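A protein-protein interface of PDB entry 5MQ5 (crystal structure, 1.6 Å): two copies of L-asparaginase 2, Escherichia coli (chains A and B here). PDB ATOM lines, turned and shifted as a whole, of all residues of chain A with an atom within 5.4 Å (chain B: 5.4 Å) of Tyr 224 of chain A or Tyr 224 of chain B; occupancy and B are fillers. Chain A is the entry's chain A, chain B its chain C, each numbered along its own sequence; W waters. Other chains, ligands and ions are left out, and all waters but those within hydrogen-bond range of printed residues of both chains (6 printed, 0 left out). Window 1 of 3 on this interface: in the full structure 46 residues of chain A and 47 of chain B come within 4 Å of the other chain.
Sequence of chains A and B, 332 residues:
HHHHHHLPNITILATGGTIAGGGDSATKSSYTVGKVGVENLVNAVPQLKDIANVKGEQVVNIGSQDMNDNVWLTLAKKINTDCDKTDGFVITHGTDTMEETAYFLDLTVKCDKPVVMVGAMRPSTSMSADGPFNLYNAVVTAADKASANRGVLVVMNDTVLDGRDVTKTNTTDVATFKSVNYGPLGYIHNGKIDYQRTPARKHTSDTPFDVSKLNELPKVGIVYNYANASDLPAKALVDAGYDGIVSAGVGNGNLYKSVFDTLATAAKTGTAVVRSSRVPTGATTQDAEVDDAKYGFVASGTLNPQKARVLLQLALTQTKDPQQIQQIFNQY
OH of Tyr 226 of chain B sits at hydrogen-bond distance from N of Ile 222 of chain A (3.2 Å).
The side-chain amide oxygen of Gln 306 of chain B is in hydrogen-bond range of the side-chain hydroxyl of Tyr 224 of chain A, at 2.6 Å.
OH of Tyr 226 of chain A lies within hydrogen-bond range of N of Ile 222 of chain B, 3.2 Å away.
NE2 of Gln 306 of chain B sits close to NE of Arg 278 of chain A (3.5 Å).
The side-chain hydroxyl (OH) of Tyr 224 of chain B lies within hydrogen-bond range of the side-chain amide oxygen (OE1) of Gln 306 of chain A (2.6 Å).
The side-chain amide nitrogen (NE2) of Gln 306 of chain A lies close to the guanidinium group (NE) of Arg 278 of chain B (3.4 Å).
The backbone carbonyl oxygen of Asn 225 of chain A lies within hydrogen-bond range of the guanidinium group of Arg 278 of chain A, 3.0 Å away.
O of Asn 225 of chain B sits at hydrogen-bond distance from NH1 of Arg 278 of chain B, at 3.0 Å.
Among the printed residues, merely in contact across the chains: Ile 222 of chain A with Tyr 224 of chain B, Tyr 224 of chain A with Ile 222 of chain B, Tyr 224 of chain A with Tyr 224 of chain B and Pro 305 of chain A with Tyr 224 of chain B.
Of chain B, only Ile 222 (3.6 Å), Tyr 224 (3.5 Å) and Gln 306 (2.6 Å) come within 4 Å of Tyr 224 of chain A.
Of chain A, only Ile 222 (3.6 Å), Tyr 224 (3.5 Å), Pro 305 (3.9 Å) and Gln 306 (2.6 Å) come within 4 Å of Tyr 224 of chain B.
Printed residues of chain B within 4 Å of Arg 278 of chain A: Gln 306 (3.4 Å).
Of the printed residues of chain B, Ile 222 of chain A touches Tyr 224 and Tyr 226.
Printed residues of chain A within 4 Å of Tyr 226 of chain B: Ile 222 (3.2 Å).
Of the printed residues of chain A, Ile 222 of chain B touches Tyr 224 (3.6 Å) and Tyr 226 (3.2 Å).
The nearest residue of chain B that does not touch Tyr 224 of chain A is Pro 305 of chain B (4.03 Å).
Hydrophobic or aromatic side chains of chain A within 4 Å of the printed part of chain B: Ile 222, Tyr 224, Tyr 226 and Pro 305.
Printed residues of chain B that touch a printed residue of chain A: Ile 222, Tyr 224, Tyr 226, Arg 278 and Gln 306.
Hydrophobic or aromatic side chains of chain B within 4 Å of the printed part of chain A: Ile 222, Tyr 224 and Tyr 226.
Ile 222 of chain A touches Tyr 226 of chain B, and with the chains exchanged Tyr 226 of chain A touches Ile 222 of chain B.
Tyr 224 of chain B touches its own counterpart, Tyr 224 of chain A.
Tyr 224 of chain A touches Gln 306 of chain B, and with the chains exchanged Gln 306 of chain A touches Tyr 224 of chain B.
Pro 305 of chain A touches Tyr 224 of chain B, but with the chains exchanged Tyr 224 of chain A does not touch Pro 305 of chain B (4.03 Å).
Water W5 bridges the backbone carbonyl oxygen of Ile 222 of chain B (2.7 Å) and the backbone NH of Tyr 224 of chain A (3.0 Å).
Water W4 bridges the backbone carbonyl oxygen of Ile 222 of chain A and the backbone NH of Tyr 224 of chain B.
Water W6 lies within hydrogen-bond range of OH of Tyr 224 of chain B and O of Arg 278 of chain A.
Water W1 lies within hydrogen-bond range of NE2 of Gln 306 of chain A (3.0 Å), O of Arg 278 of chain B (3.2 Å) and OH of Tyr 224 of chain B (3.5 Å).
Water W2 lies within hydrogen-bond range of NE2 of Gln 306 of chain B (3.0 Å), O of Arg 278 of chain A (3.1 Å) and OH of Tyr 224 of chain A (3.5 Å).
Water W3 lies within hydrogen-bond range of O of Arg 278 of chain B (3.0 Å) and O of Arg 278 of chain A (3.1 Å).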
ATOM      1  N   ILE A 222     -31.831 -22.716  16.809  1.00  0.00           N
ATOM      2  CA  ILE A 222     -31.437 -22.590  15.407  1.00  0.00           C
ATOM      3  C   ILE A 222     -29.977 -22.184  15.341  1.00  0.00           C
ATOM      4  O   ILE A 222     -29.570 -21.240  16.024  1.00  0.00           O
ATOM      5  CB  ILE A 222     -32.307 -21.559  14.655  1.00  0.00           C
ATOM      6  CG1 ILE A 222     -33.792 -21.945  14.739  1.00  0.00           C
ATOM      7  CG2 ILE A 222     -31.837 -21.443  13.207  1.00  0.00           C
ATOM      8  CD1 ILE A 222     -34.722 -20.885  14.129  1.00  0.00           C
ATOM      9  N   VAL A 223     -29.193 -22.877  14.511  1.00  0.00           N
ATOM     10  CA  VAL A 223     -27.797 -22.506  14.272  1.00  0.00           C
ATOM     11  C   VAL A 223     -27.612 -22.123  12.810  1.00  0.00           C
ATOM     12  O   VAL A 223     -28.234 -22.706  11.912  1.00  0.00           O
ATOM     13  CB  VAL A 223     -26.813 -23.630  14.672  1.00  0.00           C
ATOM     14  CG1 VAL A 223     -26.909 -23.907  16.159  1.00  0.00           C
ATOM     15  CG2 VAL A 223     -27.052 -24.909  13.875  1.00  0.00           C
ATOM     16  N   TYR A 224     -26.740 -21.141  12.566  1.00  0.00           N
ATOM     17  CA  TYR A 224     -26.486 -20.605  11.233  1.00  0.00           C
ATOM     18  C   TYR A 224     -25.223 -21.212  10.626  1.00  0.00           C
ATOM     19  O   TYR A 224     -24.237 -21.452  11.329  1.00  0.00           O
ATOM     20  CB  TYR A 224     -26.335 -19.083  11.305  1.00  0.00           C
ATOM     21  CG  TYR A 224     -26.724 -18.308  10.060  1.00  0.00           C
ATOM     22  CD1 TYR A 224     -28.062 -18.150   9.707  1.00  0.00           C
ATOM     23  CD2 TYR A 224     -25.751 -17.689   9.265  1.00  0.00           C
ATOM     24  CE1 TYR A 224     -28.429 -17.420   8.582  1.00  0.00           C
ATOM     25  CE2 TYR A 224     -26.108 -16.942   8.127  1.00  0.00           C
ATOM     26  CZ  TYR A 224     -27.457 -16.816   7.799  1.00  0.00           C
ATOM     27  OH  TYR A 224     -27.864 -16.096   6.700  1.00  0.00           O
ATOM     28  N   ASN A 225     -25.243 -21.425   9.311  1.00  0.00           N
ATOM     29  CA  ASN A 225     -24.077 -21.910   8.584  1.00  0.00           C
ATOM     30  C   ASN A 225     -23.561 -20.839   7.632  1.00  0.00           C
ATOM     31  O   ASN A 225     -24.338 -20.053   7.071  1.00  0.00           O
ATOM     32  CB  ASN A 225     -24.392 -23.176   7.781  1.00  0.00           C
ATOM     33  CG  ASN A 225     -24.597 -24.396   8.666  1.00  0.00           C
ATOM     34  OD1 ASN A 225     -23.668 -25.174   8.891  1.00  0.00           O
ATOM     35  ND2 ASN A 225     -25.823 -24.580   9.154  1.00  0.00           N
ATOM     36  N   TYR A 226     -22.239 -20.836   7.445  1.00  0.00           N
ATOM     37  CA  TYR A 226     -21.504 -19.847   6.662  1.00  0.00           C
ATOM     38  C   TYR A 226     -20.068 -20.354   6.579  1.00  0.00           C
ATOM     39  O   TYR A 226     -19.715 -21.342   7.222  1.00  0.00           O
ATOM     40  CB  TYR A 226     -21.585 -18.465   7.314  1.00  0.00           C
ATOM     41  CG  TYR A 226     -21.238 -18.475   8.796  1.00  0.00           C
ATOM     42  CD1 TYR A 226     -22.159 -18.911   9.744  1.00  0.00           C
ATOM     43  CD2 TYR A 226     -19.994 -18.047   9.236  1.00  0.00           C
ATOM     44  CE1 TYR A 226     -21.849 -18.936  11.084  1.00  0.00           C
ATOM     45  CE2 TYR A 226     -19.674 -18.051  10.582  1.00  0.00           C
ATOM     46  CZ  TYR A 226     -20.617 -18.502  11.504  1.00  0.00           C
ATOM     47  OH  TYR A 226     -20.327 -18.524  12.846  1.00  0.00           O
ATOM     48  N   ALA A 229     -17.708 -21.571   9.761  1.00  0.00           N
ATOM     49  CA  ALA A 229     -18.665 -21.483  10.858  1.00  0.00           C
ATOM     50  C   ALA A 229     -18.174 -22.203  12.107  1.00  0.00           C
ATOM     51  O   ALA A 229     -17.696 -23.339  12.052  1.00  0.00           O
ATOM     52  CB  ALA A 229     -20.014 -22.065  10.430  1.00  0.00           C
ATOM     53  N   ALA A 248     -29.843 -23.699   9.904  1.00  0.00           N
ATOM     54  CA  ALA A 248     -29.980 -22.796   8.763  1.00  0.00           C
ATOM     55  C   ALA A 248     -28.788 -23.076   7.863  1.00  0.00           C
ATOM     56  O   ALA A 248     -27.744 -22.436   7.966  1.00  0.00           O
ATOM     57  CB  ALA A 248     -30.027 -21.341   9.212  1.00  0.00           C
ATOM     58  N   VAL A 259     -19.939 -27.946  12.055  1.00  0.00           N
ATOM     59  CA  VAL A 259     -21.337 -28.006  12.471  1.00  0.00           C
ATOM     60  C   VAL A 259     -21.932 -29.374  12.156  1.00  0.00           C
ATOM     61  O   VAL A 259     -22.661 -29.950  12.969  1.00  0.00           O
ATOM     62  CB  VAL A 259     -22.129 -26.870  11.794  1.00  0.00           C
ATOM     63  CG1 VAL A 259     -23.610 -26.915  12.200  1.00  0.00           C
ATOM     64  CG2 VAL A 259     -21.492 -25.519  12.151  1.00  0.00           C
ATOM     65  N   ARG A 278     -30.640 -21.205   5.130  1.00  0.00           N
ATOM     66  CA  ARG A 278     -30.639 -19.739   5.144  1.00  0.00           C
ATOM     67  C   ARG A 278     -31.094 -19.135   3.821  1.00  0.00           C
ATOM     68  O   ARG A 278     -31.361 -17.927   3.764  1.00  0.00           O
ATOM     69  CB  ARG A 278     -29.237 -19.215   5.448  1.00  0.00           C
ATOM     70  CG  ARG A 278     -28.312 -19.249   4.239  1.00  0.00           C
ATOM     71  CD  ARG A 278     -26.863 -18.938   4.651  1.00  0.00           C
ATOM     72  NE  ARG A 278     -26.037 -18.752   3.466  1.00  0.00           N
ATOM     73  CZ  ARG A 278     -24.740 -18.439   3.485  1.00  0.00           C
ATOM     74  NH1 ARG A 278     -24.088 -18.329   4.637  1.00  0.00           N
ATOM     75  NH2 ARG A 278     -24.095 -18.243   2.339  1.00  0.00           N
ATOM     76  N   PRO A 305     -35.830 -21.673   8.496  1.00  0.00           N
ATOM     77  CA  PRO A 305     -35.384 -22.187   9.807  1.00  0.00           C
ATOM     78  C   PRO A 305     -36.367 -21.923  10.940  1.00  0.00           C
ATOM     79  O   PRO A 305     -36.639 -22.835  11.736  1.00  0.00           O
ATOM     80  CB  PRO A 305     -34.045 -21.471  10.026  1.00  0.00           C
ATOM     81  CG  PRO A 305     -33.538 -21.196   8.629  1.00  0.00           C
ATOM     82  CD  PRO A 305     -34.781 -20.879   7.823  1.00  0.00           C
ATOM     83  N   GLN A 306     -36.930 -20.709  11.007  1.00  0.00           N
ATOM     84  CA  GLN A 306     -37.848 -20.364  12.086  1.00  0.00           C
ATOM     85  C   GLN A 306     -39.182 -21.095  11.947  1.00  0.00           C
ATOM     86  O   GLN A 306     -39.796 -21.435  12.963  1.00  0.00           O
ATOM     87  CB  GLN A 306     -38.029 -18.839  12.151  1.00  0.00           C
ATOM     88  CG  GLN A 306     -38.511 -18.140  10.877  1.00  0.00           C
ATOM     89  CD  GLN A 306     -37.367 -17.685   9.979  1.00  0.00           C
ATOM     90  OE1 GLN A 306     -36.230 -18.154  10.105  1.00  0.00           O
ATOM     91  NE2 GLN A 306     -37.664 -16.751   9.068  1.00  0.00           N
ATOM     92  N   ILE B 222     -21.883 -15.837  13.764  1.00  0.00           N
ATOM     93  CA  ILE B 222     -23.231 -15.378  13.436  1.00  0.00           C
ATOM     94  C   ILE B 222     -24.235 -16.100  14.324  1.00  0.00           C
ATOM     95  O   ILE B 222     -24.204 -17.333  14.425  1.00  0.00           O
ATOM     96  CB  ILE B 222     -23.573 -15.619  11.951  1.00  0.00           C
ATOM     97  CG1 ILE B 222     -22.575 -14.889  11.040  1.00  0.00           C
ATOM     98  CG2 ILE B 222     -24.985 -15.127  11.650  1.00  0.00           C
ATOM     99  CD1 ILE B 222     -22.721 -15.200   9.555  1.00  0.00           C
ATOM    100  N   VAL B 223     -25.144 -15.338  14.942  1.00  0.00           N
ATOM    101  CA  VAL B 223     -26.230 -15.905  15.744  1.00  0.00           C
ATOM    102  C   VAL B 223     -27.571 -15.526  15.130  1.00  0.00           C
ATOM    103  O   VAL B 223     -27.743 -14.425  14.593  1.00  0.00           O
ATOM    104  CB  VAL B 223     -26.162 -15.445  17.216  1.00  0.00           C
ATOM    105  CG1 VAL B 223     -24.859 -15.906  17.854  1.00  0.00           C
ATOM    106  CG2 VAL B 223     -26.309 -13.928  17.339  1.00  0.00           C
ATOM    107  N   TYR B 224     -28.525 -16.445  15.212  1.00  0.00           N
ATOM    108  CA  TYR B 224     -29.841 -16.284  14.605  1.00  0.00           C
ATOM    109  C   TYR B 224     -30.844 -15.798  15.645  1.00  0.00           C
ATOM    110  O   TYR B 224     -30.789 -16.206  16.812  1.00  0.00           O
ATOM    111  CB  TYR B 224     -30.320 -17.623  14.025  1.00  0.00           C
ATOM    112  CG  TYR B 224     -31.259 -17.540  12.838  1.00  0.00           C
ATOM    113  CD1 TYR B 224     -30.811 -17.064  11.615  1.00  0.00           C
ATOM    114  CD2 TYR B 224     -32.585 -17.965  12.932  1.00  0.00           C
ATOM    115  CE1 TYR B 224     -31.646 -17.007  10.520  1.00  0.00           C
ATOM    116  CE2 TYR B 224     -33.436 -17.899  11.843  1.00  0.00           C
ATOM    117  CZ  TYR B 224     -32.958 -17.419  10.631  1.00  0.00           C
ATOM    118  OH  TYR B 224     -33.796 -17.370   9.549  1.00  0.00           O
ATOM    119  N   ASN B 225     -31.789 -14.968  15.212  1.00  0.00           N
ATOM    120  CA  ASN B 225     -32.900 -14.547  16.054  1.00  0.00           C
ATOM    121  C   ASN B 225     -34.218 -15.090  15.527  1.00  0.00           C
ATOM    122  O   ASN B 225     -34.416 -15.237  14.315  1.00  0.00           O
ATOM    123  CB  ASN B 225     -33.001 -13.024  16.142  1.00  0.00           C
ATOM    124  CG  ASN B 225     -31.863 -12.422  16.927  1.00  0.00           C
ATOM    125  OD1 ASN B 225     -31.997 -12.125  18.122  1.00  0.00           O
ATOM    126  ND2 ASN B 225     -30.720 -12.253  16.266  1.00  0.00           N
ATOM    127  N   TYR B 226     -35.124 -15.337  16.466  1.00  0.00           N
ATOM    128  CA  TYR B 226     -36.396 -16.008  16.236  1.00  0.00           C
ATOM    129  C   TYR B 226     -37.143 -15.955  17.564  1.00  0.00           C
ATOM    130  O   TYR B 226     -36.594 -15.518  18.580  1.00  0.00           O
ATOM    131  CB  TYR B 226     -36.193 -17.444  15.742  1.00  0.00           C
ATOM    132  CG  TYR B 226     -35.252 -18.265  16.601  1.00  0.00           C
ATOM    133  CD1 TYR B 226     -33.870 -18.147  16.474  1.00  0.00           C
ATOM    134  CD2 TYR B 226     -35.749 -19.163  17.532  1.00  0.00           C
ATOM    135  CE1 TYR B 226     -33.012 -18.891  17.257  1.00  0.00           C
ATOM    136  CE2 TYR B 226     -34.903 -19.920  18.318  1.00  0.00           C
ATOM    137  CZ  TYR B 226     -33.535 -19.781  18.176  1.00  0.00           C
ATOM    138  OH  TYR B 226     -32.691 -20.528  18.978  1.00  0.00           O
ATOM    139  N   ALA B 229     -35.714 -17.143  21.286  1.00  0.00           N
ATOM    140  CA  ALA B 229     -34.332 -17.492  20.957  1.00  0.00           C
ATOM    141  C   ALA B 229     -33.472 -17.665  22.205  1.00  0.00           C
ATOM    142  O   ALA B 229     -33.479 -16.826  23.111  1.00  0.00           O
ATOM    143  CB  ALA B 229     -33.712 -16.426  20.052  1.00  0.00           C
ATOM    144  N   ALA B 248     -28.071 -12.163  13.047  1.00  0.00           N
ATOM    145  CA  ALA B 248     -29.107 -12.279  12.022  1.00  0.00           C
ATOM    146  C   ALA B 248     -30.411 -11.964  12.733  1.00  0.00           C
ATOM    147  O   ALA B 248     -31.080 -12.845  13.284  1.00  0.00           O
ATOM    148  CB  ALA B 248     -29.116 -13.666  11.388  1.00  0.00           C
ATOM    149  N   VAL B 259     -30.791 -12.387  23.677  1.00  0.00           N
ATOM    150  CA  VAL B 259     -29.647 -12.209  22.793  1.00  0.00           C
ATOM    151  C   VAL B 259     -29.148 -10.775  22.867  1.00  0.00           C
ATOM    152  O   VAL B 259     -27.942 -10.531  22.969  1.00  0.00           O
ATOM    153  CB  VAL B 259     -30.043 -12.608  21.360  1.00  0.00           C
ATOM    154  CG1 VAL B 259     -28.863 -12.503  20.410  1.00  0.00           C
ATOM    155  CG2 VAL B 259     -30.624 -14.026  21.364  1.00  0.00           C
ATOM    156  N   ARG B 278     -32.028 -11.590   9.302  1.00  0.00           N
ATOM    157  CA  ARG B 278     -32.396 -12.790   8.555  1.00  0.00           C
ATOM    158  C   ARG B 278     -33.327 -12.506   7.377  1.00  0.00           C
ATOM    159  O   ARG B 278     -33.523 -13.390   6.536  1.00  0.00           O
ATOM    160  CB  ARG B 278     -33.070 -13.799   9.497  1.00  0.00           C
ATOM    161  CG  ARG B 278     -34.546 -13.452   9.788  1.00  0.00           C
ATOM    162  CD  ARG B 278     -35.162 -14.289  10.919  1.00  0.00           C
ATOM    163  NE  ARG B 278     -36.611 -14.091  10.947  1.00  0.00           N
ATOM    164  CZ  ARG B 278     -37.441 -14.671  11.814  1.00  0.00           C
ATOM    165  NH1 ARG B 278     -36.968 -15.466  12.767  1.00  0.00           N
ATOM    166  NH2 ARG B 278     -38.751 -14.445  11.732  1.00  0.00           N
ATOM    167  N   PRO B 305     -26.282 -11.465   6.824  1.00  0.00           N
ATOM    168  CA  PRO B 305     -25.393 -11.806   7.953  1.00  0.00           C
ATOM    169  C   PRO B 305     -24.039 -12.344   7.520  1.00  0.00           C
ATOM    170  O   PRO B 305     -23.009 -11.903   8.056  1.00  0.00           O
ATOM    171  CB  PRO B 305     -26.220 -12.837   8.744  1.00  0.00           C
ATOM    172  CG  PRO B 305     -27.648 -12.458   8.427  1.00  0.00           C
ATOM    173  CD  PRO B 305     -27.623 -12.066   6.984  1.00  0.00           C
ATOM    174  N   GLN B 306     -24.013 -13.244   6.528  1.00  0.00           N
ATOM    175  CA  GLN B 306     -22.741 -13.808   6.095  1.00  0.00           C
ATOM    176  C   GLN B 306     -21.891 -12.770   5.360  1.00  0.00           C
ATOM    177  O   GLN B 306     -20.660 -12.821   5.449  1.00  0.00           O
ATOM    178  CB  GLN B 306     -22.987 -15.066   5.243  1.00  0.00           C
ATOM    179  CG  GLN B 306     -23.884 -14.873   4.009  1.00  0.00           C
ATOM    180  CD  GLN B 306     -25.377 -15.082   4.283  1.00  0.00           C
ATOM    181  OE1 GLN B 306     -25.826 -15.034   5.422  1.00  0.00           O
ATOM    182  NE2 GLN B 306     -26.147 -15.310   3.226  1.00  0.00           N
HETATM  183  O   HOH W   1     -35.652 -15.649   7.169  1.00  0.00           O
HETATM  184  O   HOH W   2     -29.086 -15.815   3.481  1.00  0.00           O
HETATM  185  O   HOH W   3     -32.953 -15.268   4.209  1.00  0.00           O
HETATM  186  O   HOH W   4     -27.859 -19.092  16.374  1.00  0.00           O
HETATM  187  O   HOH W   5     -25.562 -19.664  14.873  1.00  0.00           O
HETATM  188  O   HOH W   6     -32.540 -17.717   6.977  1.00  0.00           O
